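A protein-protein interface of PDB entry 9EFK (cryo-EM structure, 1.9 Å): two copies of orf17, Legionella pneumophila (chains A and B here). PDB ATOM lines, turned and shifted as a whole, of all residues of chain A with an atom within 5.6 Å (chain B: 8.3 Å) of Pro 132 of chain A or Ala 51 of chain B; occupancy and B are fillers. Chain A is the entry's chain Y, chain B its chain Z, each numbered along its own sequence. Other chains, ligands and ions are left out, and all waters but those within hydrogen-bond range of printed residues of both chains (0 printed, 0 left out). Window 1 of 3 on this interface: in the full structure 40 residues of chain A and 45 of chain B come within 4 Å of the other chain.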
ATOM      1  N   ALA A   7      -3.587 -14.042  31.961  1.00  0.00           N
ATOM      2  CA  ALA A   7      -4.993 -14.325  31.746  1.00  0.00           C
ATOM      3  C   ALA A   7      -5.749 -14.404  33.070  1.00  0.00           C
ATOM      4  O   ALA A   7      -5.142 -14.526  34.134  1.00  0.00           O
ATOM      5  CB  ALA A   7      -5.138 -15.630  30.973  1.00  0.00           C
ATOM      6  N   TRP A 130      -8.178 -22.706  32.587  1.00  0.00           N
ATOM      7  CA  TRP A 130      -8.746 -22.333  31.298  1.00  0.00           C
ATOM      8  C   TRP A 130      -7.672 -21.744  30.388  1.00  0.00           C
ATOM      9  O   TRP A 130      -6.846 -20.951  30.841  1.00  0.00           O
ATOM     10  CB  TRP A 130      -9.865 -21.312  31.470  1.00  0.00           C
ATOM     11  CG  TRP A 130     -11.100 -21.831  32.115  1.00  0.00           C
ATOM     12  CD1 TRP A 130     -11.294 -23.070  32.636  1.00  0.00           C
ATOM     13  CD2 TRP A 130     -12.326 -21.121  32.303  1.00  0.00           C
ATOM     14  NE1 TRP A 130     -12.561 -23.176  33.143  1.00  0.00           N
ATOM     15  CE2 TRP A 130     -13.217 -21.992  32.949  1.00  0.00           C
ATOM     16  CE3 TRP A 130     -12.758 -19.832  31.985  1.00  0.00           C
ATOM     17  CZ2 TRP A 130     -14.510 -21.619  33.284  1.00  0.00           C
ATOM     18  CZ3 TRP A 130     -14.039 -19.463  32.320  1.00  0.00           C
ATOM     19  CH2 TRP A 130     -14.901 -20.353  32.961  1.00  0.00           C
ATOM     20  N   PRO A 131      -7.664 -22.110  29.105  1.00  0.00           N
ATOM     21  CA  PRO A 131      -6.847 -21.374  28.147  1.00  0.00           C
ATOM     22  C   PRO A 131      -7.355 -19.950  28.000  1.00  0.00           C
ATOM     23  O   PRO A 131      -8.566 -19.700  28.105  1.00  0.00           O
ATOM     24  CB  PRO A 131      -7.026 -22.169  26.842  1.00  0.00           C
ATOM     25  CG  PRO A 131      -7.564 -23.477  27.250  1.00  0.00           C
ATOM     26  CD  PRO A 131      -8.358 -23.245  28.483  1.00  0.00           C
ATOM     27  N   PRO A 132      -6.469 -18.991  27.768  1.00  0.00           N
ATOM     28  CA  PRO A 132      -6.893 -17.587  27.686  1.00  0.00           C
ATOM     29  C   PRO A 132      -7.934 -17.337  26.606  1.00  0.00           C
ATOM     30  O   PRO A 132      -8.892 -16.592  26.855  1.00  0.00           O
ATOM     31  CB  PRO A 132      -5.581 -16.848  27.393  1.00  0.00           C
ATOM     32  CG  PRO A 132      -4.567 -17.689  28.030  1.00  0.00           C
ATOM     33  CD  PRO A 132      -5.005 -19.109  27.838  1.00  0.00           C
ATOM     34  N   PRO A 133      -7.808 -17.914  25.397  1.00  0.00           N
ATOM     35  CA  PRO A 133      -8.877 -17.691  24.406  1.00  0.00           C
ATOM     36  C   PRO A 133     -10.232 -18.174  24.875  1.00  0.00           C
ATOM     37  O   PRO A 133     -11.248 -17.540  24.575  1.00  0.00           O
ATOM     38  CB  PRO A 133      -8.394 -18.478  23.183  1.00  0.00           C
ATOM     39  CG  PRO A 133      -6.965 -18.571  23.343  1.00  0.00           C
ATOM     40  CD  PRO A 133      -6.710 -18.690  24.798  1.00  0.00           C
ATOM     41  N   PHE A 134     -10.273 -19.289  25.599  1.00  0.00           N
ATOM     42  CA  PHE A 134     -11.535 -19.782  26.131  1.00  0.00           C
ATOM     43  C   PHE A 134     -12.101 -18.832  27.177  1.00  0.00           C
ATOM     44  O   PHE A 134     -13.320 -18.658  27.267  1.00  0.00           O
ATOM     45  CB  PHE A 134     -11.338 -21.181  26.712  1.00  0.00           C
ATOM     46  CG  PHE A 134     -12.584 -21.791  27.275  1.00  0.00           C
ATOM     47  CD1 PHE A 134     -13.450 -22.504  26.468  1.00  0.00           C
ATOM     48  CD2 PHE A 134     -12.877 -21.674  28.620  1.00  0.00           C
ATOM     49  CE1 PHE A 134     -14.590 -23.069  26.991  1.00  0.00           C
ATOM     50  CE2 PHE A 134     -14.016 -22.237  29.143  1.00  0.00           C
ATOM     51  CZ  PHE A 134     -14.871 -22.937  28.331  1.00  0.00           C
ATOM     52  N   SER A 135     -11.233 -18.214  27.981  1.00  0.00           N
ATOM     53  CA  SER A 135     -11.705 -17.277  28.994  1.00  0.00           C
ATOM     54  C   SER A 135     -12.410 -16.089  28.358  1.00  0.00           C
ATOM     55  O   SER A 135     -13.494 -15.689  28.794  1.00  0.00           O
ATOM     56  CB  SER A 135     -10.538 -16.805  29.860  1.00  0.00           C
ATOM     57  OG  SER A 135     -10.049 -17.846  30.678  1.00  0.00           O
ATOM     58  N   LEU A 136     -11.818 -15.522  27.307  1.00  0.00           N
ATOM     59  CA  LEU A 136     -12.442 -14.388  26.639  1.00  0.00           C
ATOM     60  C   LEU A 136     -13.715 -14.797  25.911  1.00  0.00           C
ATOM     61  O   LEU A 136     -14.637 -13.989  25.784  1.00  0.00           O
ATOM     62  CB  LEU A 136     -11.457 -13.732  25.674  1.00  0.00           C
ATOM     63  CG  LEU A 136     -11.907 -12.418  25.034  1.00  0.00           C
ATOM     64  CD1 LEU A 136     -12.509 -11.485  26.060  1.00  0.00           C
ATOM     65  CD2 LEU A 136     -10.738 -11.745  24.356  1.00  0.00           C
ATOM     66  N   TYR A 137     -13.785 -16.038  25.430  1.00  0.00           N
ATOM     67  CA  TYR A 137     -15.021 -16.522  24.829  1.00  0.00           C
ATOM     68  C   TYR A 137     -16.143 -16.601  25.856  1.00  0.00           C
ATOM     69  O   TYR A 137     -17.283 -16.235  25.563  1.00  0.00           O
ATOM     70  CB  TYR A 137     -14.785 -17.880  24.173  1.00  0.00           C
ATOM     71  CG  TYR A 137     -16.037 -18.693  23.963  1.00  0.00           C
ATOM     72  CD1 TYR A 137     -17.078 -18.212  23.187  1.00  0.00           C
ATOM     73  CD2 TYR A 137     -16.171 -19.951  24.529  1.00  0.00           C
ATOM     74  CE1 TYR A 137     -18.217 -18.947  22.996  1.00  0.00           C
ATOM     75  CE2 TYR A 137     -17.311 -20.695  24.342  1.00  0.00           C
ATOM     76  CZ  TYR A 137     -18.329 -20.187  23.570  1.00  0.00           C
ATOM     77  OH  TYR A 137     -19.473 -20.914  23.371  1.00  0.00           O
ATOM     78  N   TRP A 167     -14.577 -15.448  19.121  1.00  0.00           N
ATOM     79  CA  TRP A 167     -13.670 -16.062  20.078  1.00  0.00           C
ATOM     80  C   TRP A 167     -13.975 -17.531  20.299  1.00  0.00           C
ATOM     81  O   TRP A 167     -13.108 -18.257  20.783  1.00  0.00           O
ATOM     82  CB  TRP A 167     -13.701 -15.301  21.399  1.00  0.00           C
ATOM     83  CG  TRP A 167     -12.966 -14.016  21.303  1.00  0.00           C
ATOM     84  CD1 TRP A 167     -13.496 -12.767  21.337  1.00  0.00           C
ATOM     85  CD2 TRP A 167     -11.560 -13.851  21.112  1.00  0.00           C
ATOM     86  NE1 TRP A 167     -12.509 -11.831  21.196  1.00  0.00           N
ATOM     87  CE2 TRP A 167     -11.308 -12.472  21.053  1.00  0.00           C
ATOM     88  CE3 TRP A 167     -10.487 -14.739  20.991  1.00  0.00           C
ATOM     89  CZ2 TRP A 167     -10.029 -11.956  20.883  1.00  0.00           C
ATOM     90  CZ3 TRP A 167      -9.222 -14.226  20.819  1.00  0.00           C
ATOM     91  CH2 TRP A 167      -9.002 -12.847  20.767  1.00  0.00           C
ATOM     92  N   ARG A 170     -11.793 -19.129  17.524  1.00  0.00           N
ATOM     93  CA  ARG A 170     -10.377 -19.016  17.846  1.00  0.00           C
ATOM     94  C   ARG A 170     -10.009 -19.881  19.044  1.00  0.00           C
ATOM     95  O   ARG A 170      -8.949 -20.513  19.052  1.00  0.00           O
ATOM     96  CB  ARG A 170     -10.013 -17.557  18.090  1.00  0.00           C
ATOM     97  CG  ARG A 170     -10.279 -16.677  16.891  1.00  0.00           C
ATOM     98  CD  ARG A 170      -9.607 -15.337  17.031  1.00  0.00           C
ATOM     99  NE  ARG A 170      -8.165 -15.482  17.167  1.00  0.00           N
ATOM    100  CZ  ARG A 170      -7.309 -14.473  17.167  1.00  0.00           C
ATOM    101  NH1 ARG A 170      -7.715 -13.224  17.020  1.00  0.00           N
ATOM    102  NH2 ARG A 170      -6.014 -14.724  17.322  1.00  0.00           N
ATOM    103  N   LEU B  44      -9.589  -5.001  30.846  1.00  0.00           N
ATOM    104  CA  LEU B  44      -9.720  -5.805  29.642  1.00  0.00           C
ATOM    105  C   LEU B  44      -8.399  -6.034  28.923  1.00  0.00           C
ATOM    106  O   LEU B  44      -8.326  -6.928  28.077  1.00  0.00           O
ATOM    107  CB  LEU B  44     -10.706  -5.139  28.684  1.00  0.00           C
ATOM    108  CG  LEU B  44     -12.122  -4.973  29.225  1.00  0.00           C
ATOM    109  CD1 LEU B  44     -12.970  -4.169  28.260  1.00  0.00           C
ATOM    110  CD2 LEU B  44     -12.746  -6.326  29.489  1.00  0.00           C
ATOM    111  N   TYR B  45      -7.358  -5.267  29.245  1.00  0.00           N
ATOM    112  CA  TYR B  45      -6.102  -5.376  28.509  1.00  0.00           C
ATOM    113  C   TYR B  45      -5.486  -6.760  28.658  1.00  0.00           C
ATOM    114  O   TYR B  45      -5.104  -7.389  27.667  1.00  0.00           O
ATOM    115  CB  TYR B  45      -5.120  -4.301  28.979  1.00  0.00           C
ATOM    116  CG  TYR B  45      -3.739  -4.417  28.372  1.00  0.00           C
ATOM    117  CD1 TYR B  45      -2.755  -5.187  28.976  1.00  0.00           C
ATOM    118  CD2 TYR B  45      -3.418  -3.756  27.199  1.00  0.00           C
ATOM    119  CE1 TYR B  45      -1.504  -5.298  28.428  1.00  0.00           C
ATOM    120  CE2 TYR B  45      -2.164  -3.860  26.646  1.00  0.00           C
ATOM    121  CZ  TYR B  45      -1.212  -4.633  27.265  1.00  0.00           C
ATOM    122  OH  TYR B  45       0.041  -4.742  26.724  1.00  0.00           O
ATOM    123  N   ASP B  46      -5.365  -7.248  29.894  1.00  0.00           N
ATOM    124  CA  ASP B  46      -4.703  -8.530  30.114  1.00  0.00           C
ATOM    125  C   ASP B  46      -5.477  -9.672  29.472  1.00  0.00           C
ATOM    126  O   ASP B  46      -4.879 -10.595  28.910  1.00  0.00           O
ATOM    127  CB  ASP B  46      -4.519  -8.785  31.607  1.00  0.00           C
ATOM    128  CG  ASP B  46      -3.298  -8.092  32.167  1.00  0.00           C
ATOM    129  OD1 ASP B  46      -2.800  -7.150  31.522  1.00  0.00           O
ATOM    130  OD2 ASP B  46      -2.828  -8.495  33.251  1.00  0.00           O
ATOM    131  N   THR B  47      -6.806  -9.633  29.554  1.00  0.00           N
ATOM    132  CA  THR B  47      -7.616 -10.688  28.958  1.00  0.00           C
ATOM    133  C   THR B  47      -7.503 -10.686  27.440  1.00  0.00           C
ATOM    134  O   THR B  47      -7.379 -11.747  26.822  1.00  0.00           O
ATOM    135  CB  THR B  47      -9.073 -10.531  29.385  1.00  0.00           C
ATOM    136  OG1 THR B  47      -9.144 -10.451  30.812  1.00  0.00           O
ATOM    137  CG2 THR B  47      -9.895 -11.717  28.917  1.00  0.00           C
ATOM    138  N   LEU B  48      -7.541  -9.506  26.823  1.00  0.00           N
ATOM    139  CA  LEU B  48      -7.461  -9.426  25.370  1.00  0.00           C
ATOM    140  C   LEU B  48      -6.105  -9.897  24.864  1.00  0.00           C
ATOM    141  O   LEU B  48      -6.024 -10.719  23.947  1.00  0.00           O
ATOM    142  CB  LEU B  48      -7.737  -7.998  24.909  1.00  0.00           C
ATOM    143  CG  LEU B  48      -7.427  -7.722  23.440  1.00  0.00           C
ATOM    144  CD1 LEU B  48      -8.295  -8.577  22.534  1.00  0.00           C
ATOM    145  CD2 LEU B  48      -7.608  -6.255  23.126  1.00  0.00           C
ATOM    146  N   VAL B  49      -5.023  -9.390  25.455  1.00  0.00           N
ATOM    147  CA  VAL B  49      -3.687  -9.709  24.961  1.00  0.00           C
ATOM    148  C   VAL B  49      -3.391 -11.193  25.129  1.00  0.00           C
ATOM    149  O   VAL B  49      -2.874 -11.842  24.215  1.00  0.00           O
ATOM    150  CB  VAL B  49      -2.634  -8.836  25.666  1.00  0.00           C
ATOM    151  CG1 VAL B  49      -1.248  -9.272  25.278  1.00  0.00           C
ATOM    152  CG2 VAL B  49      -2.844  -7.383  25.312  1.00  0.00           C
ATOM    153  N   SER B  50      -3.720 -11.753  26.294  1.00  0.00           N
ATOM    154  CA  SER B  50      -3.466 -13.169  26.531  1.00  0.00           C
ATOM    155  C   SER B  50      -4.257 -14.040  25.567  1.00  0.00           C
ATOM    156  O   SER B  50      -3.743 -15.041  25.063  1.00  0.00           O
ATOM    157  CB  SER B  50      -3.796 -13.527  27.977  1.00  0.00           C
ATOM    158  OG  SER B  50      -2.959 -12.825  28.873  1.00  0.00           O
ATOM    159  N   ALA B  51      -5.510 -13.674  25.297  1.00  0.00           N
ATOM    160  CA  ALA B  51      -6.313 -14.421  24.338  1.00  0.00           C
ATOM    161  C   ALA B  51      -5.760 -14.303  22.926  1.00  0.00           C
ATOM    162  O   ALA B  51      -5.842 -15.260  22.150  1.00  0.00           O
ATOM    163  CB  ALA B  51      -7.761 -13.943  24.382  1.00  0.00           C
ATOM    164  N   GLU B  52      -5.216 -13.143  22.567  1.00  0.00           N
ATOM    165  CA  GLU B  52      -4.683 -12.956  21.223  1.00  0.00           C
ATOM    166  C   GLU B  52      -3.417 -13.773  21.013  1.00  0.00           C
ATOM    167  O   GLU B  52      -3.289 -14.495  20.020  1.00  0.00           O
ATOM    168  CB  GLU B  52      -4.408 -11.477  20.977  1.00  0.00           C
ATOM    169  CG  GLU B  52      -5.029 -10.949  19.718  1.00  0.00           C
ATOM    170  CD  GLU B  52      -4.509 -11.642  18.485  1.00  0.00           C
ATOM    171  OE1 GLU B  52      -3.321 -12.003  18.465  1.00  0.00           O
ATOM    172  OE2 GLU B  52      -5.288 -11.827  17.535  1.00  0.00           O
ATOM    173  N   LEU B  53      -2.472 -13.676  21.946  1.00  0.00           N
ATOM    174  CA  LEU B  53      -1.234 -14.432  21.839  1.00  0.00           C
ATOM    175  C   LEU B  53      -1.439 -15.914  22.110  1.00  0.00           C
ATOM    176  O   LEU B  53      -0.593 -16.724  21.726  1.00  0.00           O
ATOM    177  CB  LEU B  53      -0.189 -13.858  22.797  1.00  0.00           C
ATOM    178  CG  LEU B  53       0.262 -12.429  22.494  1.00  0.00           C
ATOM    179  CD1 LEU B  53       1.250 -11.940  23.529  1.00  0.00           C
ATOM    180  CD2 LEU B  53       0.864 -12.344  21.108  1.00  0.00           C
ATOM    181  N   GLY B  54      -2.537 -16.284  22.754  1.00  0.00           N
ATOM    182  CA  GLY B  54      -2.862 -17.663  23.027  1.00  0.00           C
ATOM    183  C   GLY B  54      -3.716 -18.347  21.987  1.00  0.00           C
ATOM    184  O   GLY B  54      -4.134 -19.487  22.203  1.00  0.00           O
ATOM    185  N   SER B  55      -3.987 -17.695  20.863  1.00  0.00           N
ATOM    186  CA  SER B  55      -4.882 -18.235  19.856  1.00  0.00           C
ATOM    187  C   SER B  55      -4.247 -18.356  18.483  1.00  0.00           C
ATOM    188  O   SER B  55      -4.903 -18.840  17.557  1.00  0.00           O
ATOM    189  CB  SER B  55      -6.137 -17.365  19.746  1.00  0.00           C
ATOM    190  OG  SER B  55      -7.284 -18.120  20.059  1.00  0.00           O
ATOM    191  N   ASN B  56      -3.003 -17.933  18.320  1.00  0.00           N
ATOM    192  CA  ASN B  56      -2.373 -17.911  17.014  1.00  0.00           C
ATOM    193  C   ASN B  56      -0.872 -18.011  17.211  1.00  0.00           C
ATOM    194  O   ASN B  56      -0.340 -17.559  18.224  1.00  0.00           O
ATOM    195  CB  ASN B  56      -2.749 -16.635  16.254  1.00  0.00           C
ATOM    196  CG  ASN B  56      -2.078 -16.539  14.912  1.00  0.00           C
ATOM    197  OD1 ASN B  56      -2.518 -17.150  13.947  1.00  0.00           O
ATOM    198  ND2 ASN B  56      -1.008 -15.764  14.840  1.00  0.00           N
ATOM    199  N   TRP B  58       2.164 -16.513  16.768  1.00  0.00           N
ATOM    200  CA  TRP B  58       2.932 -15.311  16.481  1.00  0.00           C
ATOM    201  C   TRP B  58       4.402 -15.611  16.726  1.00  0.00           C
ATOM    202  O   TRP B  58       4.767 -16.103  17.797  1.00  0.00           O
ATOM    203  CB  TRP B  58       2.485 -14.144  17.359  1.00  0.00           C
ATOM    204  CG  TRP B  58       1.085 -13.684  17.146  1.00  0.00           C
ATOM    205  CD1 TRP B  58      -0.016 -14.083  17.830  1.00  0.00           C
ATOM    206  CD2 TRP B  58       0.639 -12.711  16.200  1.00  0.00           C
ATOM    207  NE1 TRP B  58      -1.125 -13.428  17.367  1.00  0.00           N
ATOM    208  CE2 TRP B  58      -0.749 -12.580  16.362  1.00  0.00           C
ATOM    209  CE3 TRP B  58       1.278 -11.944  15.225  1.00  0.00           C
ATOM    210  CZ2 TRP B  58      -1.508 -11.714  15.588  1.00  0.00           C
ATOM    211  CZ3 TRP B  58       0.525 -11.087  14.461  1.00  0.00           C
ATOM    212  CH2 TRP B  58      -0.853 -10.976  14.648  1.00  0.00           C
ATOM    213  N   ASP B  89       4.807 -20.465  31.907  1.00  0.00           N
ATOM    214  CA  ASP B  89       4.458 -19.342  31.051  1.00  0.00           C
ATOM    215  C   ASP B  89       3.776 -19.769  29.757  1.00  0.00           C
ATOM    216  O   ASP B  89       3.491 -18.913  28.918  1.00  0.00           O
ATOM    217  CB  ASP B  89       5.701 -18.503  30.735  1.00  0.00           C
ATOM    218  CG  ASP B  89       6.784 -19.289  30.021  1.00  0.00           C
ATOM    219  OD1 ASP B  89       6.651 -20.518  29.876  1.00  0.00           O
ATOM    220  OD2 ASP B  89       7.782 -18.670  29.603  1.00  0.00           O
ATOM    221  N   CYS B  90       3.508 -21.057  29.578  1.00  0.00           N
ATOM    222  CA  CYS B  90       2.890 -21.517  28.344  1.00  0.00           C
ATOM    223  C   CYS B  90       1.453 -21.036  28.258  1.00  0.00           C
ATOM    224  O   CYS B  90       0.657 -21.234  29.179  1.00  0.00           O
ATOM    225  CB  CYS B  90       2.936 -23.036  28.243  1.00  0.00           C
ATOM    226  SG  CYS B  90       2.037 -23.687  26.818  1.00  0.00           S
ATOM    227  N   ILE B  91       1.125 -20.419  27.135  1.00  0.00           N
ATOM    228  CA  ILE B  91      -0.205 -19.888  26.905  1.00  0.00           C
ATOM    229  C   ILE B  91      -0.918 -20.607  25.764  1.00  0.00           C
ATOM    230  O   ILE B  91      -2.157 -20.577  25.716  1.00  0.00           O
ATOM    231  CB  ILE B  91      -0.136 -18.367  26.654  1.00  0.00           C
ATOM    232  CG1 ILE B  91      -1.176 -17.639  27.487  1.00  0.00           C
ATOM    233  CG2 ILE B  91      -0.222 -18.026  25.192  1.00  0.00           C
ATOM    234  CD1 ILE B  91      -0.914 -17.733  28.956  1.00  0.00           C
ATOM    235  N   MET B  92      -0.186 -21.273  24.874  1.00  0.00           N
ATOM    236  CA  MET B  92      -0.770 -22.120  23.837  1.00  0.00           C
ATOM    237  C   MET B  92       0.280 -23.133  23.413  1.00  0.00           C
ATOM    238  O   MET B  92       1.359 -22.745  22.963  1.00  0.00           O
ATOM    239  CB  MET B  92      -1.232 -21.298  22.635  1.00  0.00           C
ATOM    240  CG  MET B  92      -1.836 -22.148  21.527  1.00  0.00           C
ATOM    241  SD  MET B  92      -2.245 -21.256  20.020  1.00  0.00           S
ATOM    242  CE  MET B  92      -0.619 -20.929  19.370  1.00  0.00           C
ATOM    243  N   ASN B 124       3.115 -14.852  26.867  1.00  0.00           N
ATOM    244  CA  ASN B 124       3.034 -13.405  26.956  1.00  0.00           C
ATOM    245  C   ASN B 124       4.430 -12.806  26.886  1.00  0.00           C
ATOM    246  O   ASN B 124       5.376 -13.331  27.475  1.00  0.00           O
ATOM    247  CB  ASN B 124       2.349 -12.984  28.253  1.00  0.00           C
ATOM    248  CG  ASN B 124       0.847 -12.901  28.119  1.00  0.00           C
ATOM    249  OD1 ASN B 124       0.330 -12.204  27.253  1.00  0.00           O
ATOM    250  ND2 ASN B 124       0.139 -13.613  28.978  1.00  0.00           N
ATOM    251  N   PHE B 134       1.511  -5.191  15.164  1.00  0.00           N
ATOM    252  CA  PHE B 134       0.730  -5.868  16.189  1.00  0.00           C
ATOM    253  C   PHE B 134       0.255  -4.890  17.251  1.00  0.00           C
ATOM    254  O   PHE B 134      -0.868  -5.007  17.752  1.00  0.00           O
ATOM    255  CB  PHE B 134       1.560  -6.985  16.818  1.00  0.00           C
ATOM    256  CG  PHE B 134       0.815  -7.798  17.831  1.00  0.00           C
ATOM    257  CD1 PHE B 134       0.007  -8.843  17.434  1.00  0.00           C
ATOM    258  CD2 PHE B 134       0.934  -7.526  19.181  1.00  0.00           C
ATOM    259  CE1 PHE B 134      -0.676  -9.591  18.360  1.00  0.00           C
ATOM    260  CE2 PHE B 134       0.252  -8.273  20.110  1.00  0.00           C
ATOM    261  CZ  PHE B 134      -0.553  -9.306  19.699  1.00  0.00           C
ATOM    262  N   TYR B 137      -2.722  -3.036  15.970  1.00  0.00           N
ATOM    263  CA  TYR B 137      -3.867  -3.935  15.973  1.00  0.00           C
ATOM    264  C   TYR B 137      -4.464  -4.065  17.368  1.00  0.00           C
ATOM    265  O   TYR B 137      -5.687  -4.059  17.527  1.00  0.00           O
ATOM    266  CB  TYR B 137      -3.460  -5.300  15.427  1.00  0.00           C
ATOM    267  CG  TYR B 137      -4.393  -6.417  15.811  1.00  0.00           C
ATOM    268  CD1 TYR B 137      -5.733  -6.380  15.463  1.00  0.00           C
ATOM    269  CD2 TYR B 137      -3.930  -7.515  16.515  1.00  0.00           C
ATOM    270  CE1 TYR B 137      -6.584  -7.395  15.816  1.00  0.00           C
ATOM    271  CE2 TYR B 137      -4.774  -8.535  16.869  1.00  0.00           C
ATOM    272  CZ  TYR B 137      -6.099  -8.472  16.516  1.00  0.00           C
ATOM    273  OH  TYR B 137      -6.946  -9.488  16.868  1.00  0.00           O
ATOM    274  N   ILE B 138      -3.618  -4.181  18.390  1.00  0.00           N
ATOM    275  CA  ILE B 138      -4.116  -4.271  19.757  1.00  0.00           C
ATOM    276  C   ILE B 138      -4.801  -2.973  20.163  1.00  0.00           C
ATOM    277  O   ILE B 138      -5.809  -2.987  20.874  1.00  0.00           O
ATOM    278  CB  ILE B 138      -2.973  -4.645  20.717  1.00  0.00           C
ATOM    279  CG1 ILE B 138      -2.450  -6.044  20.400  1.00  0.00           C
ATOM    280  CG2 ILE B 138      -3.428  -4.587  22.161  1.00  0.00           C
ATOM    281  CD1 ILE B 138      -3.464  -7.134  20.601  1.00  0.00           C
ATOM    282  N   HIS B 141      -8.218  -3.100  18.609  1.00  0.00           N
ATOM    283  CA  HIS B 141      -9.053  -4.123  19.222  1.00  0.00           C
ATOM    284  C   HIS B 141      -9.470  -3.721  20.630  1.00  0.00           C
ATOM    285  O   HIS B 141     -10.628  -3.904  21.017  1.00  0.00           O
ATOM    286  CB  HIS B 141      -8.312  -5.456  19.230  1.00  0.00           C
ATOM    287  CG  HIS B 141      -9.206  -6.646  19.364  1.00  0.00           C
ATOM    288  ND1 HIS B 141      -8.900  -7.870  18.813  1.00  0.00           N
ATOM    289  CD2 HIS B 141     -10.395  -6.803  19.989  1.00  0.00           C
ATOM    290  CE1 HIS B 141      -9.862  -8.729  19.089  1.00  0.00           C
ATOM    291  NE2 HIS B 141     -10.781  -8.106  19.803  1.00  0.00           N
ATOM    292  N   MET B 145     -13.286  -2.774  22.250  1.00  0.00           N
ATOM    293  CA  MET B 145     -13.888  -3.223  23.501  1.00  0.00           C
ATOM    294  C   MET B 145     -14.267  -2.051  24.397  1.00  0.00           C
ATOM    295  O   MET B 145     -15.235  -2.146  25.156  1.00  0.00           O
ATOM    296  CB  MET B 145     -12.939  -4.173  24.230  1.00  0.00           C
ATOM    297  CG  MET B 145     -12.591  -5.414  23.428  1.00  0.00           C
ATOM    298  SD  MET B 145     -11.447  -6.534  24.249  1.00  0.00           S
ATOM    299  CE  MET B 145     -12.537  -7.319  25.424  1.00  0.00           C
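2 positions are printed for both chains.
Printed residues of chain B within 4 Å of Ala 7 of chain A: Ser 50 (3.4 Å).
Of chain B, only Ala 51 (3.7 Å), Gly 54 (3.2 Å) and Ser 55 (3.3 Å) come within 4 Å of Pro 133 of chain A.
Of the printed residues of chain B, Leu 136 of chain A touches Thr 47 (3.9 Å) and Ala 51 (3.7 Å).
Of the printed residues of chain A, Asn 56 of chain B touches Arg 170.
Printed residues of chain A within 4 Å of Ile 91 of chain B: Pro 132 (3.4 Å).
Phe 134 of chain B touches none of the printed residues of chain A.
The nearest residue of chain B that does not touch Pro 132 of chain A is Thr 47 of chain B (5.1 Å).
The nearest residue of chain A that does not touch Ala 51 of chain B is Arg 170 of chain A (4.9 Å).
The guanidinium group (NH1) of Arg 170 of chain A lies within salt-bridge range of the side-chain carboxylate (OE2) of Glu 52 of chain B.
N of Ala 7 of chain A lies within hydrogen-bond range of OG of Ser 50 of chain B (3.4 Å).
OG of Ser 55 of chain B sits at hydrogen-bond distance from O of Arg 170 of chain A, at 3.1 Å.
Of the 24 printed residues of chain B, 10 touch a printed residue of chain A.
Printed residues of chain B that touch a printed residue of chain A: Thr 47, Ser 50, Ala 51, Glu 52, Gly 54, Ser 55, Asn 56, Ile 91, Tyr 137 and His 141.
Among the printed residues, 15 pairs touch across the chains.
Among the printed residues, Asp or Glu carboxylates within 4 Å of a Lys or Arg side-chain nitrogen of the other chain: Arg 170 of chain A with Glu 52 of chain B (2.8 Å).
O of Ser 50 of chain B touches CB of Pro 132 of chain A (3.5 Å).
Ala 51 of chain B touches Pro 132 of chain A (CB to O, 3.8 Å).
Ile 91 of chain B touches Pro 132 of chain A (CG1 to CG, 3.4 Å).
Pro 133 of chain A touches Ala 51 of chain B (CG to O, 3.7 Å).
Gly 54 of chain B touches Pro 133 of chain A.
Pro 133 of chain A touches Ser 55 of chain B.
Leu 136 of chain A touches Thr 47 of chain B (CD1 to CG2, 3.9 Å).
Ala 51 of chain B touches Trp 167 of chain A (O to CZ3, 3.8 Å).
Trp 167 of chain A touches His 141 of chain B (CZ2 to CE1, 3.7 Å).
Tyr 137 of chain B touches Arg 170 of chain A.
ND1 of His 141 of chain B is in hydrogen-bond range of OH of Tyr 137 of chain B, at 3.2 Å.
The indole nitrogen (NE1) of Trp 58 of chain B lies close to the side-chain amide nitrogen (ND2) of Asn 56 of chain B (3.4 Å).
The side-chain amide nitrogen of Asn 124 of chain B lies within hydrogen-bond range of the side-chain hydroxyl of Ser 50 of chain B (3.2 Å).
The backbone carbonyl oxygen (O) of Asp 46 of chain B lies within hydrogen-bond range of the side-chain hydroxyl (OG) of Ser 50 of chain B (2.9 Å).
NE1 of Trp 58 of chain B sits at hydrogen-bond distance from OE1 of Glu 52 of chain B, 2.8 Å away.
The side-chain carboxylate (OE2) of Glu 52 of chain B is in hydrogen-bond range of the side-chain hydroxyl (OH) of Tyr 137 of chain B (2.9 Å).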
